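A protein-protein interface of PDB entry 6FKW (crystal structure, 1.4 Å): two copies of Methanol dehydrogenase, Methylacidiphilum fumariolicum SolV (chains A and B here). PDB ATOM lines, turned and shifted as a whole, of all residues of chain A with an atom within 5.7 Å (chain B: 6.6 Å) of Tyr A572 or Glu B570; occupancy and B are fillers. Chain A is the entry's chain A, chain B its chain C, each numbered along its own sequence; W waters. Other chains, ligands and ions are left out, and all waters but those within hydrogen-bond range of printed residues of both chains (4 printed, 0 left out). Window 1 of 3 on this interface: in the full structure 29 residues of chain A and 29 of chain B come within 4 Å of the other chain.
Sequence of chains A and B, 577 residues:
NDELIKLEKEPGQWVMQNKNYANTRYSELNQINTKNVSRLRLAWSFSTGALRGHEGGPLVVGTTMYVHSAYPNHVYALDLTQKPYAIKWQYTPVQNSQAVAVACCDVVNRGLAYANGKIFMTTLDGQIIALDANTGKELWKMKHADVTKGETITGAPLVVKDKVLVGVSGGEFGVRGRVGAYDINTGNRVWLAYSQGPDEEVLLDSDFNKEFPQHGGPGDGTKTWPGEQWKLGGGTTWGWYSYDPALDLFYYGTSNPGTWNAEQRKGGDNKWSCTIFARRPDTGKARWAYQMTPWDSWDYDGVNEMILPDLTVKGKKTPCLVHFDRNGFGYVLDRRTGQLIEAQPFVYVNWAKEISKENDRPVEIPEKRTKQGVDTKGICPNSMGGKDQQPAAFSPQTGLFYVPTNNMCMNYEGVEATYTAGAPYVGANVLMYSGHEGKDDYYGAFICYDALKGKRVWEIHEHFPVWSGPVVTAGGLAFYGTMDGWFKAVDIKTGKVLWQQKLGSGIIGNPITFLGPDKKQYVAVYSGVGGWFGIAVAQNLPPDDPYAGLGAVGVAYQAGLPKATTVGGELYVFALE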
ATOM      1  N   LEU A  42     -19.215  -9.773 -11.077  1.00  0.00           N
ATOM      2  CA  LEU A  42     -18.895  -8.548 -10.352  1.00  0.00           C
ATOM      3  C   LEU A  42     -18.504  -7.457 -11.342  1.00  0.00           C
ATOM      4  O   LEU A  42     -17.646  -7.669 -12.201  1.00  0.00           O
ATOM      5  CB  LEU A  42     -17.765  -8.775  -9.345  1.00  0.00           C
ATOM      6  CG  LEU A  42     -17.506  -7.597  -8.388  1.00  0.00           C
ATOM      7  CD1 LEU A  42     -18.685  -7.363  -7.466  1.00  0.00           C
ATOM      8  CD2 LEU A  42     -16.255  -7.838  -7.561  1.00  0.00           C
ATOM      9  N   TRP A  44     -18.087  -3.986 -10.000  1.00  0.00           N
ATOM     10  CA  TRP A  44     -17.180  -3.204  -9.168  1.00  0.00           C
ATOM     11  C   TRP A  44     -17.483  -3.406  -7.689  1.00  0.00           C
ATOM     12  O   TRP A  44     -18.506  -3.967  -7.324  1.00  0.00           O
ATOM     13  CB  TRP A  44     -17.227  -1.712  -9.535  1.00  0.00           C
ATOM     14  CG  TRP A  44     -18.585  -1.008  -9.538  1.00  0.00           C
ATOM     15  CD1 TRP A  44     -19.455  -0.890 -10.595  1.00  0.00           C
ATOM     16  CD2 TRP A  44     -19.201  -0.312  -8.442  1.00  0.00           C
ATOM     17  NE1 TRP A  44     -20.565  -0.175 -10.216  1.00  0.00           N
ATOM     18  CE2 TRP A  44     -20.438   0.193  -8.902  1.00  0.00           C
ATOM     19  CE3 TRP A  44     -18.831  -0.071  -7.111  1.00  0.00           C
ATOM     20  CZ2 TRP A  44     -21.305   0.926  -8.082  1.00  0.00           C
ATOM     21  CZ3 TRP A  44     -19.697   0.661  -6.296  1.00  0.00           C
ATOM     22  CH2 TRP A  44     -20.918   1.149  -6.788  1.00  0.00           C
ATOM     23  N   SER A  45     -16.575  -2.946  -6.839  1.00  0.00           N
ATOM     24  CA  SER A  45     -16.786  -3.016  -5.401  1.00  0.00           C
ATOM     25  C   SER A  45     -16.218  -1.770  -4.741  1.00  0.00           C
ATOM     26  O   SER A  45     -15.468  -1.014  -5.359  1.00  0.00           O
ATOM     27  CB  SER A  45     -16.178  -4.295  -4.810  1.00  0.00           C
ATOM     28  OG  SER A  45     -14.812  -4.420  -5.137  1.00  0.00           O
ATOM     29  N   PHE A  46     -16.595  -1.579  -3.481  1.00  0.00           N
ATOM     30  CA  PHE A  46     -16.236  -0.387  -2.721  1.00  0.00           C
ATOM     31  C   PHE A  46     -16.161  -0.760  -1.247  1.00  0.00           C
ATOM     32  O   PHE A  46     -17.129  -1.267  -0.690  1.00  0.00           O
ATOM     33  CB  PHE A  46     -17.274   0.712  -2.945  1.00  0.00           C
ATOM     34  CG  PHE A  46     -17.094   1.905  -2.055  1.00  0.00           C
ATOM     35  CD1 PHE A  46     -16.040   2.785  -2.251  1.00  0.00           C
ATOM     36  CD2 PHE A  46     -17.975   2.140  -1.014  1.00  0.00           C
ATOM     37  CE1 PHE A  46     -15.876   3.884  -1.422  1.00  0.00           C
ATOM     38  CE2 PHE A  46     -17.817   3.236  -0.184  1.00  0.00           C
ATOM     39  CZ  PHE A  46     -16.766   4.105  -0.392  1.00  0.00           C
ATOM     40  N   LEU A 503     -18.560 -14.384  -1.508  1.00  0.00           N
ATOM     41  CA  LEU A 503     -17.971 -13.087  -1.200  1.00  0.00           C
ATOM     42  C   LEU A 503     -17.099 -13.203   0.047  1.00  0.00           C
ATOM     43  O   LEU A 503     -17.008 -14.273   0.650  1.00  0.00           O
ATOM     44  CB  LEU A 503     -19.078 -12.049  -0.999  1.00  0.00           C
ATOM     45  CG  LEU A 503     -20.137 -12.006  -2.107  1.00  0.00           C
ATOM     46  CD1 LEU A 503     -21.047 -10.805  -1.934  1.00  0.00           C
ATOM     47  CD2 LEU A 503     -19.453 -11.981  -3.462  1.00  0.00           C
ATOM     48  N   GLY A 504     -16.465 -12.101   0.428  1.00  0.00           N
ATOM     49  CA  GLY A 504     -15.390 -12.155   1.411  1.00  0.00           C
ATOM     50  C   GLY A 504     -15.781 -12.279   2.868  1.00  0.00           C
ATOM     51  O   GLY A 504     -14.944 -12.655   3.691  1.00  0.00           O
ATOM     52  N   SER A 505     -17.032 -11.962   3.191  1.00  0.00           N
ATOM     53  CA  SER A 505     -17.531 -12.028   4.562  1.00  0.00           C
ATOM     54  C   SER A 505     -19.015 -12.355   4.515  1.00  0.00           C
ATOM     55  O   SER A 505     -19.681 -12.102   3.504  1.00  0.00           O
ATOM     56  CB  SER A 505     -17.306 -10.683   5.269  1.00  0.00           C
ATOM     57  OG  SER A 505     -17.709 -10.709   6.633  1.00  0.00           O
ATOM     58  N   VAL A 523     -27.045  -5.111  -9.478  1.00  0.00           N
ATOM     59  CA  VAL A 523     -27.491  -5.644  -8.192  1.00  0.00           C
ATOM     60  C   VAL A 523     -26.354  -5.395  -7.209  1.00  0.00           C
ATOM     61  O   VAL A 523     -25.212  -5.744  -7.494  1.00  0.00           O
ATOM     62  CB  VAL A 523     -27.794  -7.157  -8.277  1.00  0.00           C
ATOM     63  CG1 VAL A 523     -28.213  -7.702  -6.917  1.00  0.00           C
ATOM     64  CG2 VAL A 523     -28.868  -7.424  -9.323  1.00  0.00           C
ATOM     65  N   ALA A 524     -26.665  -4.792  -6.064  1.00  0.00           N
ATOM     66  CA  ALA A 524     -25.637  -4.401  -5.095  1.00  0.00           C
ATOM     67  C   ALA A 524     -25.969  -4.948  -3.720  1.00  0.00           C
ATOM     68  O   ALA A 524     -27.138  -5.027  -3.346  1.00  0.00           O
ATOM     69  CB  ALA A 524     -25.517  -2.890  -5.034  1.00  0.00           C
ATOM     70  N   VAL A 525     -24.942  -5.323  -2.964  1.00  0.00           N
ATOM     71  CA  VAL A 525     -25.149  -5.829  -1.610  1.00  0.00           C
ATOM     72  C   VAL A 525     -23.923  -5.563  -0.741  1.00  0.00           C
ATOM     73  O   VAL A 525     -22.791  -5.560  -1.231  1.00  0.00           O
ATOM     74  CB  VAL A 525     -25.478  -7.334  -1.633  1.00  0.00           C
ATOM     75  CG1 VAL A 525     -24.255  -8.162  -1.983  1.00  0.00           C
ATOM     76  CG2 VAL A 525     -26.100  -7.787  -0.321  1.00  0.00           C
ATOM     77  N   TYR A 526     -24.162  -5.339   0.547  1.00  0.00           N
ATOM     78  CA  TYR A 526     -23.077  -5.281   1.524  1.00  0.00           C
ATOM     79  C   TYR A 526     -22.664  -6.672   1.977  1.00  0.00           C
ATOM     80  O   TYR A 526     -23.507  -7.553   2.147  1.00  0.00           O
ATOM     81  CB  TYR A 526     -23.486  -4.533   2.790  1.00  0.00           C
ATOM     82  CG  TYR A 526     -23.833  -3.067   2.667  1.00  0.00           C
ATOM     83  CD1 TYR A 526     -23.196  -2.227   1.756  1.00  0.00           C
ATOM     84  CD2 TYR A 526     -24.801  -2.520   3.488  1.00  0.00           C
ATOM     85  CE1 TYR A 526     -23.533  -0.881   1.666  1.00  0.00           C
ATOM     86  CE2 TYR A 526     -25.138  -1.186   3.412  1.00  0.00           C
ATOM     87  CZ  TYR A 526     -24.507  -0.366   2.506  1.00  0.00           C
ATOM     88  OH  TYR A 526     -24.852   0.968   2.432  1.00  0.00           O
ATOM     89  N   SER A 527     -21.360  -6.832   2.173  1.00  0.00           N
ATOM     90  CA  SER A 527     -20.764  -7.983   2.831  1.00  0.00           C
ATOM     91  C   SER A 527     -20.109  -7.462   4.097  1.00  0.00           C
ATOM     92  O   SER A 527     -19.560  -6.361   4.105  1.00  0.00           O
ATOM     93  CB  SER A 527     -19.704  -8.590   1.912  1.00  0.00           C
ATOM     94  OG  SER A 527     -19.019  -9.678   2.496  1.00  0.00           O
ATOM     95  N   GLY A 568     -15.576  -8.055   7.894  1.00  0.00           N
ATOM     96  CA  GLY A 568     -15.297  -7.259   6.702  1.00  0.00           C
ATOM     97  C   GLY A 568     -16.273  -6.109   6.580  1.00  0.00           C
ATOM     98  O   GLY A 568     -17.054  -5.852   7.490  1.00  0.00           O
ATOM     99  N   GLY A 569     -16.228  -5.422   5.444  1.00  0.00           N
ATOM    100  CA  GLY A 569     -17.132  -4.309   5.171  1.00  0.00           C
ATOM    101  C   GLY A 569     -16.935  -3.873   3.739  1.00  0.00           C
ATOM    102  O   GLY A 569     -16.096  -3.022   3.450  1.00  0.00           O
ATOM    103  N   GLU A 570     -17.706  -4.466   2.838  1.00  0.00           N
ATOM    104  CA  GLU A 570     -17.504  -4.253   1.410  1.00  0.00           C
ATOM    105  C   GLU A 570     -18.844  -4.196   0.710  1.00  0.00           C
ATOM    106  O   GLU A 570     -19.739  -4.976   1.018  1.00  0.00           O
ATOM    107  CB  GLU A 570     -16.684  -5.400   0.824  1.00  0.00           C
ATOM    108  CG  GLU A 570     -16.076  -5.117  -0.543  1.00  0.00           C
ATOM    109  CD  GLU A 570     -14.695  -4.494  -0.471  1.00  0.00           C
ATOM    110  OE1 GLU A 570     -14.238  -4.146   0.636  1.00  0.00           O
ATOM    111  OE2 GLU A 570     -14.059  -4.353  -1.531  1.00  0.00           O
ATOM    112  N   LEU A 571     -18.971  -3.263  -0.227  1.00  0.00           N
ATOM    113  CA  LEU A 571     -20.112  -3.196  -1.134  1.00  0.00           C
ATOM    114  C   LEU A 571     -19.716  -3.875  -2.441  1.00  0.00           C
ATOM    115  O   LEU A 571     -18.707  -3.512  -3.039  1.00  0.00           O
ATOM    116  CB  LEU A 571     -20.478  -1.733  -1.382  1.00  0.00           C
ATOM    117  CG  LEU A 571     -21.493  -1.487  -2.491  1.00  0.00           C
ATOM    118  CD1 LEU A 571     -22.838  -2.080  -2.117  1.00  0.00           C
ATOM    119  CD2 LEU A 571     -21.609   0.001  -2.776  1.00  0.00           C
ATOM    120  N   TYR A 572     -20.510  -4.855  -2.871  1.00  0.00           N
ATOM    121  CA  TYR A 572     -20.277  -5.561  -4.140  1.00  0.00           C
ATOM    122  C   TYR A 572     -21.395  -5.231  -5.111  1.00  0.00           C
ATOM    123  O   TYR A 572     -22.558  -5.291  -4.738  1.00  0.00           O
ATOM    124  CB  TYR A 572     -20.276  -7.072  -3.933  1.00  0.00           C
ATOM    125  CG  TYR A 572     -19.085  -7.650  -3.203  1.00  0.00           C
ATOM    126  CD1 TYR A 572     -19.038  -7.676  -1.815  1.00  0.00           C
ATOM    127  CD2 TYR A 572     -18.010  -8.187  -3.906  1.00  0.00           C
ATOM    128  CE1 TYR A 572     -17.949  -8.216  -1.154  1.00  0.00           C
ATOM    129  CE2 TYR A 572     -16.917  -8.727  -3.250  1.00  0.00           C
ATOM    130  CZ  TYR A 572     -16.897  -8.734  -1.876  1.00  0.00           C
ATOM    131  OH  TYR A 572     -15.814  -9.273  -1.219  1.00  0.00           O
ATOM    132  N   VAL A 573     -21.041  -4.895  -6.351  1.00  0.00           N
ATOM    133  CA  VAL A 573     -22.029  -4.516  -7.359  1.00  0.00           C
ATOM    134  C   VAL A 573     -21.865  -5.394  -8.600  1.00  0.00           C
ATOM    135  O   VAL A 573     -20.787  -5.445  -9.199  1.00  0.00           O
ATOM    136  CB  VAL A 573     -21.908  -3.025  -7.731  1.00  0.00           C
ATOM    137  CG1 VAL A 573     -23.018  -2.621  -8.691  1.00  0.00           C
ATOM    138  CG2 VAL A 573     -21.941  -2.168  -6.466  1.00  0.00           C
ATOM    139  N   PHE A 574     -22.950  -6.071  -8.969  1.00  0.00           N
ATOM    140  CA  PHE A 574     -22.967  -7.060 -10.040  1.00  0.00           C
ATOM    141  C   PHE A 574     -23.796  -6.586 -11.225  1.00  0.00           C
ATOM    142  O   PHE A 574     -24.735  -5.808 -11.064  1.00  0.00           O
ATOM    143  CB  PHE A 574     -23.561  -8.379  -9.532  1.00  0.00           C
ATOM    144  CG  PHE A 574     -22.790  -9.000  -8.409  1.00  0.00           C
ATOM    145  CD1 PHE A 574     -23.022  -8.613  -7.094  1.00  0.00           C
ATOM    146  CD2 PHE A 574     -21.830  -9.969  -8.666  1.00  0.00           C
ATOM    147  CE1 PHE A 574     -22.305  -9.191  -6.057  1.00  0.00           C
ATOM    148  CE2 PHE A 574     -21.110 -10.548  -7.630  1.00  0.00           C
ATOM    149  CZ  PHE A 574     -21.353 -10.154  -6.329  1.00  0.00           C
ATOM    150  N   LEU B  42     -14.191 -11.876 -11.470  1.00  0.00           N
ATOM    151  CA  LEU B  42     -14.014 -12.322 -10.098  1.00  0.00           C
ATOM    152  C   LEU B  42     -14.599 -13.722  -9.918  1.00  0.00           C
ATOM    153  O   LEU B  42     -15.744 -13.988 -10.285  1.00  0.00           O
ATOM    154  CB  LEU B  42     -14.655 -11.352  -9.100  1.00  0.00           C
ATOM    155  CG  LEU B  42     -14.262 -11.594  -7.633  1.00  0.00           C
ATOM    156  CD1 LEU B  42     -12.782 -11.331  -7.414  1.00  0.00           C
ATOM    157  CD2 LEU B  42     -15.070 -10.730  -6.680  1.00  0.00           C
ATOM    158  N   TRP B  44     -13.887 -15.466  -6.668  1.00  0.00           N
ATOM    159  CA  TRP B  44     -14.241 -15.413  -5.256  1.00  0.00           C
ATOM    160  C   TRP B  44     -13.406 -14.377  -4.542  1.00  0.00           C
ATOM    161  O   TRP B  44     -12.420 -13.885  -5.083  1.00  0.00           O
ATOM    162  CB  TRP B  44     -14.100 -16.787  -4.578  1.00  0.00           C
ATOM    163  CG  TRP B  44     -12.771 -17.527  -4.687  1.00  0.00           C
ATOM    164  CD1 TRP B  44     -12.403 -18.411  -5.664  1.00  0.00           C
ATOM    165  CD2 TRP B  44     -11.659 -17.464  -3.775  1.00  0.00           C
ATOM    166  NE1 TRP B  44     -11.139 -18.890  -5.425  1.00  0.00           N
ATOM    167  CE2 TRP B  44     -10.658 -18.330  -4.272  1.00  0.00           C
ATOM    168  CE3 TRP B  44     -11.409 -16.760  -2.591  1.00  0.00           C
ATOM    169  CZ2 TRP B  44      -9.431 -18.507  -3.626  1.00  0.00           C
ATOM    170  CZ3 TRP B  44     -10.189 -16.938  -1.952  1.00  0.00           C
ATOM    171  CH2 TRP B  44      -9.217 -17.808  -2.474  1.00  0.00           C
ATOM    172  N   SER B  45     -13.817 -14.049  -3.319  1.00  0.00           N
ATOM    173  CA  SER B  45     -13.049 -13.147  -2.469  1.00  0.00           C
ATOM    174  C   SER B  45     -13.085 -13.607  -1.015  1.00  0.00           C
ATOM    175  O   SER B  45     -13.886 -14.468  -0.631  1.00  0.00           O
ATOM    176  CB  SER B  45     -13.553 -11.705  -2.593  1.00  0.00           C
ATOM    177  OG  SER B  45     -14.936 -11.638  -2.322  1.00  0.00           O
ATOM    178  N   PHE B  46     -12.199 -13.018  -0.218  1.00  0.00           N
ATOM    179  CA  PHE B  46     -12.036 -13.377   1.180  1.00  0.00           C
ATOM    180  C   PHE B  46     -11.568 -12.145   1.954  1.00  0.00           C
ATOM    181  O   PHE B  46     -10.557 -11.540   1.596  1.00  0.00           O
ATOM    182  CB  PHE B  46     -11.024 -14.519   1.303  1.00  0.00           C
ATOM    183  CG  PHE B  46     -10.629 -14.830   2.723  1.00  0.00           C
ATOM    184  CD1 PHE B  46     -11.518 -15.450   3.581  1.00  0.00           C
ATOM    185  CD2 PHE B  46      -9.367 -14.490   3.192  1.00  0.00           C
ATOM    186  CE1 PHE B  46     -11.156 -15.734   4.888  1.00  0.00           C
ATOM    187  CE2 PHE B  46      -9.001 -14.771   4.498  1.00  0.00           C
ATOM    188  CZ  PHE B  46      -9.898 -15.392   5.343  1.00  0.00           C
ATOM    189  N   SER B  47     -12.298 -11.778   3.001  1.00  0.00           N
ATOM    190  CA  SER B  47     -11.915 -10.636   3.830  1.00  0.00           C
ATOM    191  C   SER B  47     -10.838 -11.050   4.816  1.00  0.00           C
ATOM    192  O   SER B  47     -10.946 -12.093   5.459  1.00  0.00           O
ATOM    193  CB  SER B  47     -13.110 -10.096   4.606  1.00  0.00           C
ATOM    194  OG  SER B  47     -12.721  -8.983   5.399  1.00  0.00           O
ATOM    195  N   THR B  48      -9.803 -10.225   4.937  1.00  0.00           N
ATOM    196  CA  THR B  48      -8.705 -10.516   5.852  1.00  0.00           C
ATOM    197  C   THR B  48      -9.059 -10.183   7.299  1.00  0.00           C
ATOM    198  O   THR B  48      -8.335 -10.574   8.213  1.00  0.00           O
ATOM    199  CB  THR B  48      -7.445  -9.711   5.500  1.00  0.00           C
ATOM    200  OG1 THR B  48      -7.706  -8.318   5.728  1.00  0.00           O
ATOM    201  CG2 THR B  48      -7.031  -9.946   4.044  1.00  0.00           C
ATOM    202  N   GLY B  49     -10.153  -9.455   7.513  1.00  0.00           N
ATOM    203  CA  GLY B  49     -10.582  -9.101   8.859  1.00  0.00           C
ATOM    204  C   GLY B  49      -9.786  -7.974   9.488  1.00  0.00           C
ATOM    205  O   GLY B  49      -9.873  -7.760  10.689  1.00  0.00           O
ATOM    206  N   ALA B  50      -9.012  -7.259   8.678  1.00  0.00           N
ATOM    207  CA  ALA B  50      -8.248  -6.104   9.141  1.00  0.00           C
ATOM    208  C   ALA B  50      -8.368  -4.952   8.154  1.00  0.00           C
ATOM    209  O   ALA B  50      -8.706  -5.153   6.986  1.00  0.00           O
ATOM    210  CB  ALA B  50      -6.787  -6.474   9.337  1.00  0.00           C
ATOM    211  N   HIS B  54      -2.456  -3.573   3.091  1.00  0.00           N
ATOM    212  CA  HIS B  54      -2.274  -5.001   2.848  1.00  0.00           C
ATOM    213  C   HIS B  54      -1.211  -5.245   1.784  1.00  0.00           C
ATOM    214  O   HIS B  54      -1.492  -5.266   0.580  1.00  0.00           O
ATOM    215  CB  HIS B  54      -3.615  -5.656   2.520  1.00  0.00           C
ATOM    216  CG  HIS B  54      -4.439  -5.908   3.739  1.00  0.00           C
ATOM    217  ND1 HIS B  54      -5.006  -4.893   4.479  1.00  0.00           N
ATOM    218  CD2 HIS B  54      -4.769  -7.061   4.367  1.00  0.00           C
ATOM    219  CE1 HIS B  54      -5.660  -5.411   5.502  1.00  0.00           C
ATOM    220  NE2 HIS B  54      -5.531  -6.726   5.456  1.00  0.00           N
ATOM    221  N   VAL B 525      -5.040 -11.098  -5.587  1.00  0.00           N
ATOM    222  CA  VAL B 525      -4.392  -9.878  -5.112  1.00  0.00           C
ATOM    223  C   VAL B 525      -5.108  -9.326  -3.881  1.00  0.00           C
ATOM    224  O   VAL B 525      -6.331  -9.445  -3.759  1.00  0.00           O
ATOM    225  CB  VAL B 525      -4.351  -8.804  -6.230  1.00  0.00           C
ATOM    226  CG1 VAL B 525      -5.739  -8.249  -6.514  1.00  0.00           C
ATOM    227  CG2 VAL B 525      -3.375  -7.693  -5.885  1.00  0.00           C
ATOM    228  N   TYR B 526      -4.337  -8.725  -2.978  1.00  0.00           N
ATOM    229  CA  TYR B 526      -4.908  -8.018  -1.842  1.00  0.00           C
ATOM    230  C   TYR B 526      -5.338  -6.615  -2.244  1.00  0.00           C
ATOM    231  O   TYR B 526      -4.666  -5.955  -3.031  1.00  0.00           O
ATOM    232  CB  TYR B 526      -3.885  -7.840  -0.726  1.00  0.00           C
ATOM    233  CG  TYR B 526      -3.412  -9.079  -0.007  1.00  0.00           C
ATOM    234  CD1 TYR B 526      -4.242 -10.178   0.212  1.00  0.00           C
ATOM    235  CD2 TYR B 526      -2.118  -9.140   0.471  1.00  0.00           C
ATOM    236  CE1 TYR B 526      -3.779 -11.302   0.882  1.00  0.00           C
ATOM    237  CE2 TYR B 526      -1.650 -10.258   1.143  1.00  0.00           C
ATOM    238  CZ  TYR B 526      -2.479 -11.332   1.347  1.00  0.00           C
ATOM    239  OH  TYR B 526      -2.004 -12.444   2.017  1.00  0.00           O
ATOM    240  N   SER B 527      -6.456  -6.184  -1.677  1.00  0.00           N
ATOM    241  CA  SER B 527      -6.896  -4.796  -1.717  1.00  0.00           C
ATOM    242  C   SER B 527      -6.927  -4.278  -0.285  1.00  0.00           C
ATOM    243  O   SER B 527      -7.283  -5.006   0.642  1.00  0.00           O
ATOM    244  CB  SER B 527      -8.286  -4.729  -2.348  1.00  0.00           C
ATOM    245  OG  SER B 527      -8.869  -3.441  -2.263  1.00  0.00           O
ATOM    246  N   GLY B 528      -6.552  -3.019  -0.107  1.00  0.00           N
ATOM    247  CA  GLY B 528      -6.485  -2.419   1.222  1.00  0.00           C
ATOM    248  C   GLY B 528      -5.360  -1.419   1.235  1.00  0.00           C
ATOM    249  O   GLY B 528      -4.189  -1.781   1.392  1.00  0.00           O
ATOM    250  N   GLY B 568      -9.555  -0.737   3.614  1.00  0.00           N
ATOM    251  CA  GLY B 568     -10.178  -2.044   3.443  1.00  0.00           C
ATOM    252  C   GLY B 568      -9.175  -3.142   3.724  1.00  0.00           C
ATOM    253  O   GLY B 568      -8.082  -2.879   4.225  1.00  0.00           O
ATOM    254  N   GLY B 569      -9.548  -4.372   3.401  1.00  0.00           N
ATOM    255  CA  GLY B 569      -8.672  -5.525   3.585  1.00  0.00           C
ATOM    256  C   GLY B 569      -9.361  -6.736   2.992  1.00  0.00           C
ATOM    257  O   GLY B 569     -10.115  -7.429   3.673  1.00  0.00           O
ATOM    258  N   GLU B 570      -9.103  -6.981   1.712  1.00  0.00           N
ATOM    259  CA  GLU B 570      -9.831  -8.000   0.971  1.00  0.00           C
ATOM    260  C   GLU B 570      -8.904  -8.695  -0.005  1.00  0.00           C
ATOM    261  O   GLU B 570      -8.097  -8.047  -0.668  1.00  0.00           O
ATOM    262  CB  GLU B 570     -10.979  -7.359   0.188  1.00  0.00           C
ATOM    263  CG  GLU B 570     -12.044  -8.340  -0.283  1.00  0.00           C
ATOM    264  CD  GLU B 570     -13.146  -8.560   0.735  1.00  0.00           C
ATOM    265  OE1 GLU B 570     -13.047  -8.038   1.865  1.00  0.00           O
ATOM    266  OE2 GLU B 570     -14.119  -9.260   0.400  1.00  0.00           O
ATOM    267  N   LEU B 571      -9.030 -10.016  -0.085  1.00  0.00           N
ATOM    268  CA  LEU B 571      -8.357 -10.820  -1.096  1.00  0.00           C
ATOM    269  C   LEU B 571      -9.341 -11.085  -2.231  1.00  0.00           C
ATOM    270  O   LEU B 571     -10.425 -11.610  -1.994  1.00  0.00           O
ATOM    271  CB  LEU B 571      -7.902 -12.141  -0.483  1.00  0.00           C
ATOM    272  CG  LEU B 571      -7.370 -13.194  -1.455  1.00  0.00           C
ATOM    273  CD1 LEU B 571      -6.114 -12.692  -2.143  1.00  0.00           C
ATOM    274  CD2 LEU B 571      -7.119 -14.505  -0.728  1.00  0.00           C
ATOM    275  N   TYR B 572      -8.955 -10.713  -3.450  1.00  0.00           N
ATOM    276  CA  TYR B 572      -9.767 -10.939  -4.646  1.00  0.00           C
ATOM    277  C   TYR B 572      -9.089 -11.973  -5.532  1.00  0.00           C
ATOM    278  O   TYR B 572      -7.892 -11.872  -5.791  1.00  0.00           O
ATOM    279  CB  TYR B 572      -9.906  -9.652  -5.459  1.00  0.00           C
ATOM    280  CG  TYR B 572     -10.772  -8.571  -4.864  1.00  0.00           C
ATOM    281  CD1 TYR B 572     -10.257  -7.667  -3.945  1.00  0.00           C
ATOM    282  CD2 TYR B 572     -12.107  -8.441  -5.236  1.00  0.00           C
ATOM    283  CE1 TYR B 572     -11.054  -6.670  -3.408  1.00  0.00           C
ATOM    284  CE2 TYR B 572     -12.909  -7.447  -4.704  1.00  0.00           C
ATOM    285  CZ  TYR B 572     -12.374  -6.568  -3.790  1.00  0.00           C
ATOM    286  OH  TYR B 572     -13.164  -5.575  -3.258  1.00  0.00           O
HETATM  287  O   HOH W   1     -15.563  -9.531 -12.259  1.00  0.00           O
HETATM  288  O   HOH W   2     -17.947 -12.320 -10.717  1.00  0.00           O
HETATM  289  O   HOH W   3     -14.338  -6.680   3.640  1.00  0.00           O
HETATM  290  O   HOH W   4     -12.159  -4.291   2.245  1.00  0.00           O
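Leu B42 touches its own counterpart, Leu A42.
Ser A45 touches Tyr B572, and with the chains exchanged Tyr A572 touches Ser B45.
Glu A570 touches Tyr B572, and with the chains exchanged Tyr A572 touches Glu B570.
Of the 11 pairs that touch across the chains among the printed residues, 5 have their exchanged pair printed and touching as well.
Of the 19 printed residues of chain A, 7 touch a printed residue of chain B.
Hydrophobic or aromatic side chains of chain A that line the printed part of chain B: Leu A42 and Tyr A572.
Printed residues of chain B that touch a printed residue of chain A: Leu B42, Ser B45, Phe B46, Ser B47, Glu B570 and Tyr B572.
Hydrophobic or aromatic side chains of chain B that line the printed part of chain A: Leu B42 and Tyr B572.
Water W3 lies within hydrogen-bond range of the side-chain carboxylate of Glu B570, the backbone NH of Gly A569 and the side-chain hydroxyl of Ser B47.
Water W4 lies within hydrogen-bond range of OE1 of Glu A570 (2.6 Å) and N of Gly B569 (2.9 Å).
Water W1 lies within hydrogen-bond range of the backbone carbonyl oxygen (O) of Leu A42 (2.8 Å) and the backbone NH (N) of Leu B42 (2.8 Å).
Water W2 bridges the backbone carbonyl oxygen of Leu B42 (2.8 Å) and the backbone NH of Leu A42 (2.9 Å).
O of Val A525 sits at hydrogen-bond distance from N of Tyr A572 (2.9 Å).
The backbone NH (N) of Ser A527 is in hydrogen-bond range of the backbone carbonyl oxygen (O) of Glu A570, 2.7 Å away.
OG of Ser B47 lies close to N of Gly B49 (3.4 Å).
The side-chain hydroxyl (OG) of Ser B47 is in hydrogen-bond range of the backbone carbonyl oxygen (O) of Gly B569 (3.5 Å).
The backbone carbonyl oxygen (O) of Val B525 is in hydrogen-bond range of the backbone NH (N) of Tyr B572, at 2.9 Å.
The backbone carbonyl oxygen (O) of Glu B570 sits at hydrogen-bond distance from the backbone NH (N) of Ser B527, 2.7 Å away.
Among the printed residues, merely in contact across the chains: Leu A42 with Leu B42 (3.2 Å), Gly A504 with Phe B46 (3.6 Å), Gly A504 with Glu B570 (3.3 Å) and Gly A568 with Ser B47 (3.4 Å).
OG of Ser A45 is in hydrogen-bond range of OH of Tyr B572 (2.8 Å).
N of Gly A504 sits at hydrogen-bond distance from OG of Ser B45.
The backbone NH (N) of Ser B47 lies within hydrogen-bond range of the backbone carbonyl oxygen (O) of Gly A504 (2.9 Å).
The side-chain hydroxyl (OH) of Tyr A572 sits at hydrogen-bond distance from the side-chain hydroxyl (OG) of Ser B45 (2.8 Å).
The backbone carbonyl oxygen (O) of Leu A503 sits close to the backbone carbonyl oxygen (O) of Ser B45 (3.4 Å).
OE2 of Glu A570 sits close to OH of Tyr B572.
The side-chain carboxylate (OE2) of Glu B570 sits close to the side-chain hydroxyl (OH) of Tyr A572, at 2.3 Å.
Printed residues of chain B within 4 Å of Gly A504: Ser B45, Phe B46, Ser B47 and Glu B570.
Of the printed residues of chain B, Gly A568 touches Ser B47 (3.4 Å).
Tyr A572 touches just these residues of chain B: Ser B45 and Glu B570.
Of the printed residues of chain A, Ser B47 touches Gly A504 and Gly A568.
Glu B570 touches just these residues of chain A: Gly A504 and Tyr A572.
The nearest printed residue of chain B that does not touch Glu A570 is Glu B570 (4.3 Å).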
